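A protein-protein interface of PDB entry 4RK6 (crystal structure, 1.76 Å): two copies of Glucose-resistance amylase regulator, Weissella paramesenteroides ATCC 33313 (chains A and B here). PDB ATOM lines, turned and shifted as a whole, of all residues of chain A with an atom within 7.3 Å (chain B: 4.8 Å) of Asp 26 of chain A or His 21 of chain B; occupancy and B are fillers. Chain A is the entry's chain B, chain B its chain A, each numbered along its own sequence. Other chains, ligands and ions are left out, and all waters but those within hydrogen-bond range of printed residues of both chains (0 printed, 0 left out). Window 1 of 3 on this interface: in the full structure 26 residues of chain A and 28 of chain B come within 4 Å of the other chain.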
ATOM      1  N   VAL A  17      26.643  -0.776  29.098  1.00  0.00           N
ATOM      2  CA  VAL A  17      27.572  -1.895  29.130  1.00  0.00           C
ATOM      3  C   VAL A  17      28.925  -1.389  28.634  1.00  0.00           C
ATOM      4  O   VAL A  17      28.980  -0.691  27.627  1.00  0.00           O
ATOM      5  CB  VAL A  17      27.086  -3.023  28.189  1.00  0.00           C
ATOM      6  CG1 VAL A  17      28.095  -4.163  28.134  1.00  0.00           C
ATOM      7  CG2 VAL A  17      25.713  -3.531  28.621  1.00  0.00           C
ATOM      8  N   HIS A  21      34.150  -5.885  28.168  1.00  0.00           N
ATOM      9  CA  HIS A  21      33.430  -6.567  29.255  1.00  0.00           C
ATOM     10  C   HIS A  21      33.597  -8.078  29.169  1.00  0.00           C
ATOM     11  O   HIS A  21      33.739  -8.627  28.073  1.00  0.00           O
ATOM     12  CB  HIS A  21      31.934  -6.236  29.182  1.00  0.00           C
ATOM     13  CG  HIS A  21      31.282  -6.655  27.896  1.00  0.00           C
ATOM     14  ND1 HIS A  21      31.541  -6.035  26.691  1.00  0.00           N
ATOM     15  CD2 HIS A  21      30.381  -7.630  27.629  1.00  0.00           C
ATOM     16  CE1 HIS A  21      30.830  -6.612  25.739  1.00  0.00           C
ATOM     17  NE2 HIS A  21      30.115  -7.581  26.281  1.00  0.00           N
ATOM     18  N   THR A  22      33.559  -8.747  30.322  1.00  0.00           N
ATOM     19  CA  THR A  22      33.503 -10.213  30.365  1.00  0.00           C
ATOM     20  C   THR A  22      32.146 -10.645  29.773  1.00  0.00           C
ATOM     21  O   THR A  22      31.262  -9.809  29.541  1.00  0.00           O
ATOM     22  CB  THR A  22      33.681 -10.763  31.819  1.00  0.00           C
ATOM     23  OG1 THR A  22      34.904 -10.287  32.410  1.00  0.00           O
ATOM     24  CG2 THR A  22      33.709 -12.287  31.864  1.00  0.00           C
ATOM     25  N   ASN A  23      31.991 -11.944  29.520  1.00  0.00           N
ATOM     26  CA  ASN A  23      30.701 -12.531  29.133  1.00  0.00           C
ATOM     27  C   ASN A  23      29.569 -12.370  30.165  1.00  0.00           C
ATOM     28  O   ASN A  23      28.411 -12.721  29.883  1.00  0.00           O
ATOM     29  CB  ASN A  23      30.872 -14.024  28.812  1.00  0.00           C
ATOM     30  CG  ASN A  23      31.728 -14.265  27.579  1.00  0.00           C
ATOM     31  OD1 ASN A  23      31.376 -13.846  26.476  1.00  0.00           O
ATOM     32  ND2 ASN A  23      32.856 -14.951  27.758  1.00  0.00           N
ATOM     33  N   PHE A  24      29.871 -11.827  31.345  1.00  0.00           N
ATOM     34  CA  PHE A  24      28.832 -11.716  32.371  1.00  0.00           C
ATOM     35  C   PHE A  24      27.700 -10.749  31.997  1.00  0.00           C
ATOM     36  O   PHE A  24      26.569 -10.927  32.445  1.00  0.00           O
ATOM     37  CB  PHE A  24      29.424 -11.443  33.766  1.00  0.00           C
ATOM     38  CG  PHE A  24      29.721 -10.000  34.056  1.00  0.00           C
ATOM     39  CD1 PHE A  24      28.716  -9.139  34.433  1.00  0.00           C
ATOM     40  CD2 PHE A  24      31.018  -9.513  33.996  1.00  0.00           C
ATOM     41  CE1 PHE A  24      28.970  -7.818  34.727  1.00  0.00           C
ATOM     42  CE2 PHE A  24      31.284  -8.178  34.272  1.00  0.00           C
ATOM     43  CZ  PHE A  24      30.259  -7.329  34.637  1.00  0.00           C
ATOM     44  N   ALA A  25      27.986  -9.753  31.156  1.00  0.00           N
ATOM     45  CA  ALA A  25      26.977  -8.769  30.753  1.00  0.00           C
ATOM     46  C   ALA A  25      25.756  -9.415  30.128  1.00  0.00           C
ATOM     47  O   ALA A  25      24.627  -9.059  30.454  1.00  0.00           O
ATOM     48  CB  ALA A  25      27.569  -7.756  29.783  1.00  0.00           C
ATOM     49  N   ASP A  26      25.978 -10.358  29.213  1.00  0.00           N
ATOM     50  CA  ASP A  26      24.866 -11.023  28.529  1.00  0.00           C
ATOM     51  C   ASP A  26      23.972 -11.781  29.503  1.00  0.00           C
ATOM     52  O   ASP A  26      22.759 -11.826  29.327  1.00  0.00           O
ATOM     53  CB  ASP A  26      25.383 -12.012  27.458  1.00  0.00           C
ATOM     54  CG  ASP A  26      25.939 -11.313  26.219  1.00  0.00           C
ATOM     55  OD1 ASP A  26      25.795 -10.076  26.088  1.00  0.00           O
ATOM     56  OD2 ASP A  26      26.526 -12.013  25.364  1.00  0.00           O
ATOM     57  N   GLU A  27      24.584 -12.380  30.523  1.00  0.00           N
ATOM     58  CA  GLU A  27      23.821 -13.097  31.544  1.00  0.00           C
ATOM     59  C   GLU A  27      22.971 -12.141  32.390  1.00  0.00           C
ATOM     60  O   GLU A  27      21.818 -12.435  32.693  1.00  0.00           O
ATOM     61  CB  GLU A  27      24.742 -13.944  32.414  1.00  0.00           C
ATOM     62  CG  GLU A  27      25.264 -15.186  31.702  1.00  0.00           C
ATOM     63  CD  GLU A  27      24.218 -16.290  31.628  1.00  0.00           C
ATOM     64  OE1 GLU A  27      23.988 -16.974  32.657  1.00  0.00           O
ATOM     65  OE2 GLU A  27      23.623 -16.462  30.549  1.00  0.00           O
ATOM     66  N   ILE A  28      23.538 -11.000  32.765  1.00  0.00           N
ATOM     67  CA  ILE A  28      22.754  -9.970  33.453  1.00  0.00           C
ATOM     68  C   ILE A  28      21.596  -9.486  32.597  1.00  0.00           C
ATOM     69  O   ILE A  28      20.461  -9.368  33.077  1.00  0.00           O
ATOM     70  CB  ILE A  28      23.643  -8.770  33.875  1.00  0.00           C
ATOM     71  CG1 ILE A  28      24.625  -9.230  34.952  1.00  0.00           C
ATOM     72  CG2 ILE A  28      22.778  -7.610  34.359  1.00  0.00           C
ATOM     73  CD1 ILE A  28      25.549  -8.161  35.477  1.00  0.00           C
ATOM     74  N   ILE A  29      21.878  -9.217  31.323  1.00  0.00           N
ATOM     75  CA  ILE A  29      20.886  -8.735  30.368  1.00  0.00           C
ATOM     76  C   ILE A  29      19.745  -9.728  30.131  1.00  0.00           C
ATOM     77  O   ILE A  29      18.607  -9.323  29.958  1.00  0.00           O
ATOM     78  CB  ILE A  29      21.541  -8.337  29.030  1.00  0.00           C
ATOM     79  CG1 ILE A  29      22.313  -7.030  29.209  1.00  0.00           C
ATOM     80  CG2 ILE A  29      20.499  -8.154  27.928  1.00  0.00           C
ATOM     81  CD1 ILE A  29      23.353  -6.799  28.137  1.00  0.00           C
ATOM     82  N   LYS A  30      20.060 -11.019  30.141  1.00  0.00           N
ATOM     83  CA  LYS A  30      19.041 -12.065  30.037  1.00  0.00           C
ATOM     84  C   LYS A  30      18.027 -11.924  31.179  1.00  0.00           C
ATOM     85  O   LYS A  30      16.804 -12.001  30.966  1.00  0.00           O
ATOM     86  CB  LYS A  30      19.728 -13.434  30.047  1.00  0.00           C
ATOM     87  CG  LYS A  30      18.831 -14.649  29.873  1.00  0.00           C
ATOM     88  CD  LYS A  30      19.680 -15.884  29.589  1.00  0.00           C
ATOM     89  CE  LYS A  30      18.985 -17.172  30.001  1.00  0.00           C
ATOM     90  NZ  LYS A  30      18.948 -17.336  31.480  1.00  0.00           N
ATOM     91  N   GLY A  31      18.529 -11.690  32.390  1.00  0.00           N
ATOM     92  CA  GLY A  31      17.665 -11.448  33.555  1.00  0.00           C
ATOM     93  C   GLY A  31      16.874 -10.150  33.467  1.00  0.00           C
ATOM     94  O   GLY A  31      15.680 -10.121  33.747  1.00  0.00           O
ATOM     95  N   LEU A  32      17.535  -9.057  33.080  1.00  0.00           N
ATOM     96  CA  LEU A  32      16.842  -7.784  32.879  1.00  0.00           C
ATOM     97  C   LEU A  32      15.725  -7.916  31.853  1.00  0.00           C
ATOM     98  O   LEU A  32      14.614  -7.418  32.026  1.00  0.00           O
ATOM     99  CB  LEU A  32      17.806  -6.703  32.385  1.00  0.00           C
ATOM    100  CG  LEU A  32      18.824  -6.101  33.328  1.00  0.00           C
ATOM    101  CD1 LEU A  32      19.654  -5.080  32.551  1.00  0.00           C
ATOM    102  CD2 LEU A  32      18.123  -5.439  34.503  1.00  0.00           C
ATOM    103  N   TYR A  47      26.539   0.921  24.580  1.00  0.00           N
ATOM    104  CA  TYR A  47      27.896   0.620  24.988  1.00  0.00           C
ATOM    105  C   TYR A  47      28.616   1.927  25.380  1.00  0.00           C
ATOM    106  O   TYR A  47      28.261   3.013  24.905  1.00  0.00           O
ATOM    107  CB  TYR A  47      28.658  -0.158  23.894  1.00  0.00           C
ATOM    108  CG  TYR A  47      28.188  -1.590  23.746  1.00  0.00           C
ATOM    109  CD1 TYR A  47      27.130  -1.920  22.900  1.00  0.00           C
ATOM    110  CD2 TYR A  47      28.790  -2.613  24.465  1.00  0.00           C
ATOM    111  CE1 TYR A  47      26.694  -3.232  22.777  1.00  0.00           C
ATOM    112  CE2 TYR A  47      28.364  -3.925  24.348  1.00  0.00           C
ATOM    113  CZ  TYR A  47      27.316  -4.229  23.504  1.00  0.00           C
ATOM    114  OH  TYR A  47      26.895  -5.533  23.391  1.00  0.00           O
ATOM    115  N   LEU A  73      26.437  -1.357  34.624  1.00  0.00           N
ATOM    116  CA  LEU A  73      27.187  -2.580  34.908  1.00  0.00           C
ATOM    117  C   LEU A  73      28.686  -2.306  35.171  1.00  0.00           C
ATOM    118  O   LEU A  73      29.389  -3.179  35.680  1.00  0.00           O
ATOM    119  CB  LEU A  73      27.081  -3.521  33.707  1.00  0.00           C
ATOM    120  CG  LEU A  73      25.826  -4.361  33.581  1.00  0.00           C
ATOM    121  CD1 LEU A  73      24.606  -3.495  33.325  1.00  0.00           C
ATOM    122  CD2 LEU A  73      26.024  -5.362  32.454  1.00  0.00           C
ATOM    123  N   PHE A 244      24.059 -14.182  37.731  1.00  0.00           N
ATOM    124  CA  PHE A 244      23.936 -12.950  36.984  1.00  0.00           C
ATOM    125  C   PHE A 244      22.493 -12.675  36.518  1.00  0.00           C
ATOM    126  O   PHE A 244      22.014 -11.561  36.630  1.00  0.00           O
ATOM    127  CB  PHE A 244      24.931 -12.913  35.807  1.00  0.00           C
ATOM    128  CG  PHE A 244      26.373 -12.834  36.237  1.00  0.00           C
ATOM    129  CD1 PHE A 244      26.863 -11.698  36.909  1.00  0.00           C
ATOM    130  CD2 PHE A 244      27.255 -13.874  35.964  1.00  0.00           C
ATOM    131  CE1 PHE A 244      28.190 -11.645  37.332  1.00  0.00           C
ATOM    132  CE2 PHE A 244      28.589 -13.811  36.357  1.00  0.00           C
ATOM    133  CZ  PHE A 244      29.069 -12.695  37.027  1.00  0.00           C
ATOM    134  N   PRO A 245      21.780 -13.697  36.015  1.00  0.00           N
ATOM    135  CA  PRO A 245      20.388 -13.402  35.667  1.00  0.00           C
ATOM    136  C   PRO A 245      19.545 -12.905  36.845  1.00  0.00           C
ATOM    137  O   PRO A 245      18.729 -12.013  36.654  1.00  0.00           O
ATOM    138  CB  PRO A 245      19.852 -14.751  35.155  1.00  0.00           C
ATOM    139  CG  PRO A 245      21.061 -15.489  34.698  1.00  0.00           C
ATOM    140  CD  PRO A 245      22.175 -15.065  35.622  1.00  0.00           C
ATOM    141  N   VAL B  17      19.601  -7.883  17.530  1.00  0.00           N
ATOM    142  CA  VAL B  17      20.418  -9.052  17.854  1.00  0.00           C
ATOM    143  C   VAL B  17      19.505 -10.163  18.401  1.00  0.00           C
ATOM    144  O   VAL B  17      18.628  -9.894  19.216  1.00  0.00           O
ATOM    145  CB  VAL B  17      21.455  -8.696  18.935  1.00  0.00           C
ATOM    146  CG1 VAL B  17      22.396  -9.860  19.220  1.00  0.00           C
ATOM    147  CG2 VAL B  17      22.243  -7.455  18.517  1.00  0.00           C
ATOM    148  N   PRO B  18      19.692 -11.395  17.935  1.00  0.00           N
ATOM    149  CA  PRO B  18      18.902 -12.490  18.528  1.00  0.00           C
ATOM    150  C   PRO B  18      19.274 -12.744  19.991  1.00  0.00           C
ATOM    151  O   PRO B  18      20.433 -12.568  20.381  1.00  0.00           O
ATOM    152  CB  PRO B  18      19.253 -13.706  17.663  1.00  0.00           C
ATOM    153  CG  PRO B  18      20.526 -13.372  16.976  1.00  0.00           C
ATOM    154  CD  PRO B  18      20.687 -11.877  16.957  1.00  0.00           C
ATOM    155  N   LEU B  19      18.298 -13.132  20.806  1.00  0.00           N
ATOM    156  CA  LEU B  19      18.591 -13.482  22.203  1.00  0.00           C
ATOM    157  C   LEU B  19      19.641 -14.596  22.286  1.00  0.00           C
ATOM    158  O   LEU B  19      20.539 -14.551  23.129  1.00  0.00           O
ATOM    159  CB  LEU B  19      17.328 -13.901  22.960  1.00  0.00           C
ATOM    160  CG  LEU B  19      16.685 -12.875  23.904  1.00  0.00           C
ATOM    161  CD1 LEU B  19      15.647 -13.595  24.749  1.00  0.00           C
ATOM    162  CD2 LEU B  19      17.698 -12.162  24.797  1.00  0.00           C
ATOM    163  N   ILE B  20      19.525 -15.577  21.396  1.00  0.00           N
ATOM    164  CA  ILE B  20      20.455 -16.702  21.323  1.00  0.00           C
ATOM    165  C   ILE B  20      21.472 -16.470  20.200  1.00  0.00           C
ATOM    166  O   ILE B  20      21.159 -16.653  19.018  1.00  0.00           O
ATOM    167  CB  ILE B  20      19.693 -18.023  21.065  1.00  0.00           C
ATOM    168  CG1 ILE B  20      18.638 -18.259  22.156  1.00  0.00           C
ATOM    169  CG2 ILE B  20      20.662 -19.200  20.990  1.00  0.00           C
ATOM    170  CD1 ILE B  20      17.537 -19.213  21.743  1.00  0.00           C
ATOM    171  N   HIS B  21      22.690 -16.083  20.566  1.00  0.00           N
ATOM    172  CA  HIS B  21      23.714 -15.752  19.573  1.00  0.00           C
ATOM    173  C   HIS B  21      25.097 -16.228  19.994  1.00  0.00           C
ATOM    174  O   HIS B  21      25.423 -16.219  21.184  1.00  0.00           O
ATOM    175  CB  HIS B  21      23.747 -14.235  19.331  1.00  0.00           C
ATOM    176  CG  HIS B  21      23.991 -13.424  20.571  1.00  0.00           C
ATOM    177  ND1 HIS B  21      23.020 -13.218  21.529  1.00  0.00           N
ATOM    178  CD2 HIS B  21      25.091 -12.759  21.004  1.00  0.00           C
ATOM    179  CE1 HIS B  21      23.512 -12.466  22.499  1.00  0.00           C
ATOM    180  NE2 HIS B  21      24.765 -12.172  22.203  1.00  0.00           N
ATOM    181  N   THR B  22      25.901 -16.641  19.010  1.00  0.00           N
ATOM    182  CA  THR B  22      27.341 -16.827  19.207  1.00  0.00           C
ATOM    183  C   THR B  22      27.916 -15.449  19.584  1.00  0.00           C
ATOM    184  O   THR B  22      27.226 -14.416  19.469  1.00  0.00           O
ATOM    185  CB  THR B  22      28.041 -17.380  17.923  1.00  0.00           C
ATOM    186  OG1 THR B  22      27.467 -18.636  17.516  1.00  0.00           O
ATOM    187  CG2 THR B  22      29.532 -17.595  18.132  1.00  0.00           C
ATOM    188  N   ASN B  23      29.166 -15.425  20.039  1.00  0.00           N
ATOM    189  CA  ASN B  23      29.867 -14.163  20.273  1.00  0.00           C
ATOM    190  C   ASN B  23      30.202 -13.342  19.020  1.00  0.00           C
ATOM    191  O   ASN B  23      30.880 -12.309  19.128  1.00  0.00           O
ATOM    192  CB  ASN B  23      31.141 -14.387  21.109  1.00  0.00           C
ATOM    193  CG  ASN B  23      30.901 -14.220  22.602  1.00  0.00           C
ATOM    194  OD1 ASN B  23      30.070 -13.412  23.034  1.00  0.00           O
ATOM    195  ND2 ASN B  23      31.645 -14.973  23.402  1.00  0.00           N
ATOM    196  N   ALA B  25      28.212 -11.487  17.420  1.00  0.00           N
ATOM    197  CA  ALA B  25      27.447 -10.228  17.470  1.00  0.00           C
ATOM    198  C   ALA B  25      28.265  -9.064  18.009  1.00  0.00           C
ATOM    199  O   ALA B  25      28.268  -7.972  17.432  1.00  0.00           O
ATOM    200  CB  ALA B  25      26.188 -10.406  18.311  1.00  0.00           C
ATOM    201  N   TYR B  47      17.309  -6.604  21.553  1.00  0.00           N
ATOM    202  CA  TYR B  47      17.260  -8.048  21.367  1.00  0.00           C
ATOM    203  C   TYR B  47      15.895  -8.484  20.857  1.00  0.00           C
ATOM    204  O   TYR B  47      14.875  -7.803  21.060  1.00  0.00           O
ATOM    205  CB  TYR B  47      17.618  -8.793  22.655  1.00  0.00           C
ATOM    206  CG  TYR B  47      19.067  -8.635  23.028  1.00  0.00           C
ATOM    207  CD1 TYR B  47      20.053  -9.391  22.411  1.00  0.00           C
ATOM    208  CD2 TYR B  47      19.461  -7.708  23.990  1.00  0.00           C
ATOM    209  CE1 TYR B  47      21.389  -9.246  22.747  1.00  0.00           C
ATOM    210  CE2 TYR B  47      20.797  -7.550  24.328  1.00  0.00           C
ATOM    211  CZ  TYR B  47      21.757  -8.324  23.705  1.00  0.00           C
ATOM    212  OH  TYR B  47      23.086  -8.181  24.031  1.00  0.00           O
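The side-chain amide nitrogen (ND2) of Asn 23 of chain B sits at hydrogen-bond distance from the side-chain amide oxygen (OD1) of Asn 23 of chain A (3.3 Å).
The backbone carbonyl oxygen of Pro 18 of chain B lies within hydrogen-bond range of a ring nitrogen (ND1) of His 21 of chain B, 2.9 Å away.
O of Leu 19 of chain B is in hydrogen-bond range of ND1 of His 21 of chain B (3.2 Å).
Among the printed residues, merely in contact across the chains: Asp 26 of chain A with His 21 of chain B (3.6 Å), Asp 26 of chain A with Tyr 47 of chain B (3.9 Å) and Ile 29 of chain A with Tyr 47 of chain B (3.7 Å).
Asn 23 of chain B touches its own counterpart, Asn 23 of chain A.
Of the 4 pairs that touch across the chains among the printed residues, 1 has its exchanged pair printed and touching as well.
Of the 17 printed residues of chain A, 3 touch a printed residue of chain B.
Printed residues of chain A that touch a printed residue of chain B: Asn 23, Asp 26 and Ile 29.
Hydrophobic or aromatic side chains of chain A that line the printed part of chain B: Ile 29.
Along chain A the printed residues that touch a printed residue of chain B span positions 23 to 29.
Printed residues of chain B that touch a printed residue of chain A: His 21, Asn 23 and Tyr 47.
Hydrophobic or aromatic side chains of chain B that line the printed part of chain A: His 21 and Tyr 47.
Among the printed residues, 4 pairs touch across the chains.
Among the printed residues, no Asp or Glu carboxylate lies within 4 Å of a Lys or Arg side-chain nitrogen of the other chain.
Of chain B, only His 21 (3.6 Å) and Tyr 47 (3.9 Å) come within 4 Å of Asp 26 of chain A.
Of chain A, only Asp 26 (3.6 Å) comes within 4 Å of His 21 of chain B.
Printed residues of chain A within 4 Å of Asn 23 of chain B: Asn 23 (3.3 Å).
Of the printed residues of chain A, Tyr 47 of chain B touches Asp 26 and Ile 29.
Of the printed residues of chain B, Ile 29 of chain A touches Tyr 47.
Phe 24 of chain A touches none of the printed residues of chain B.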
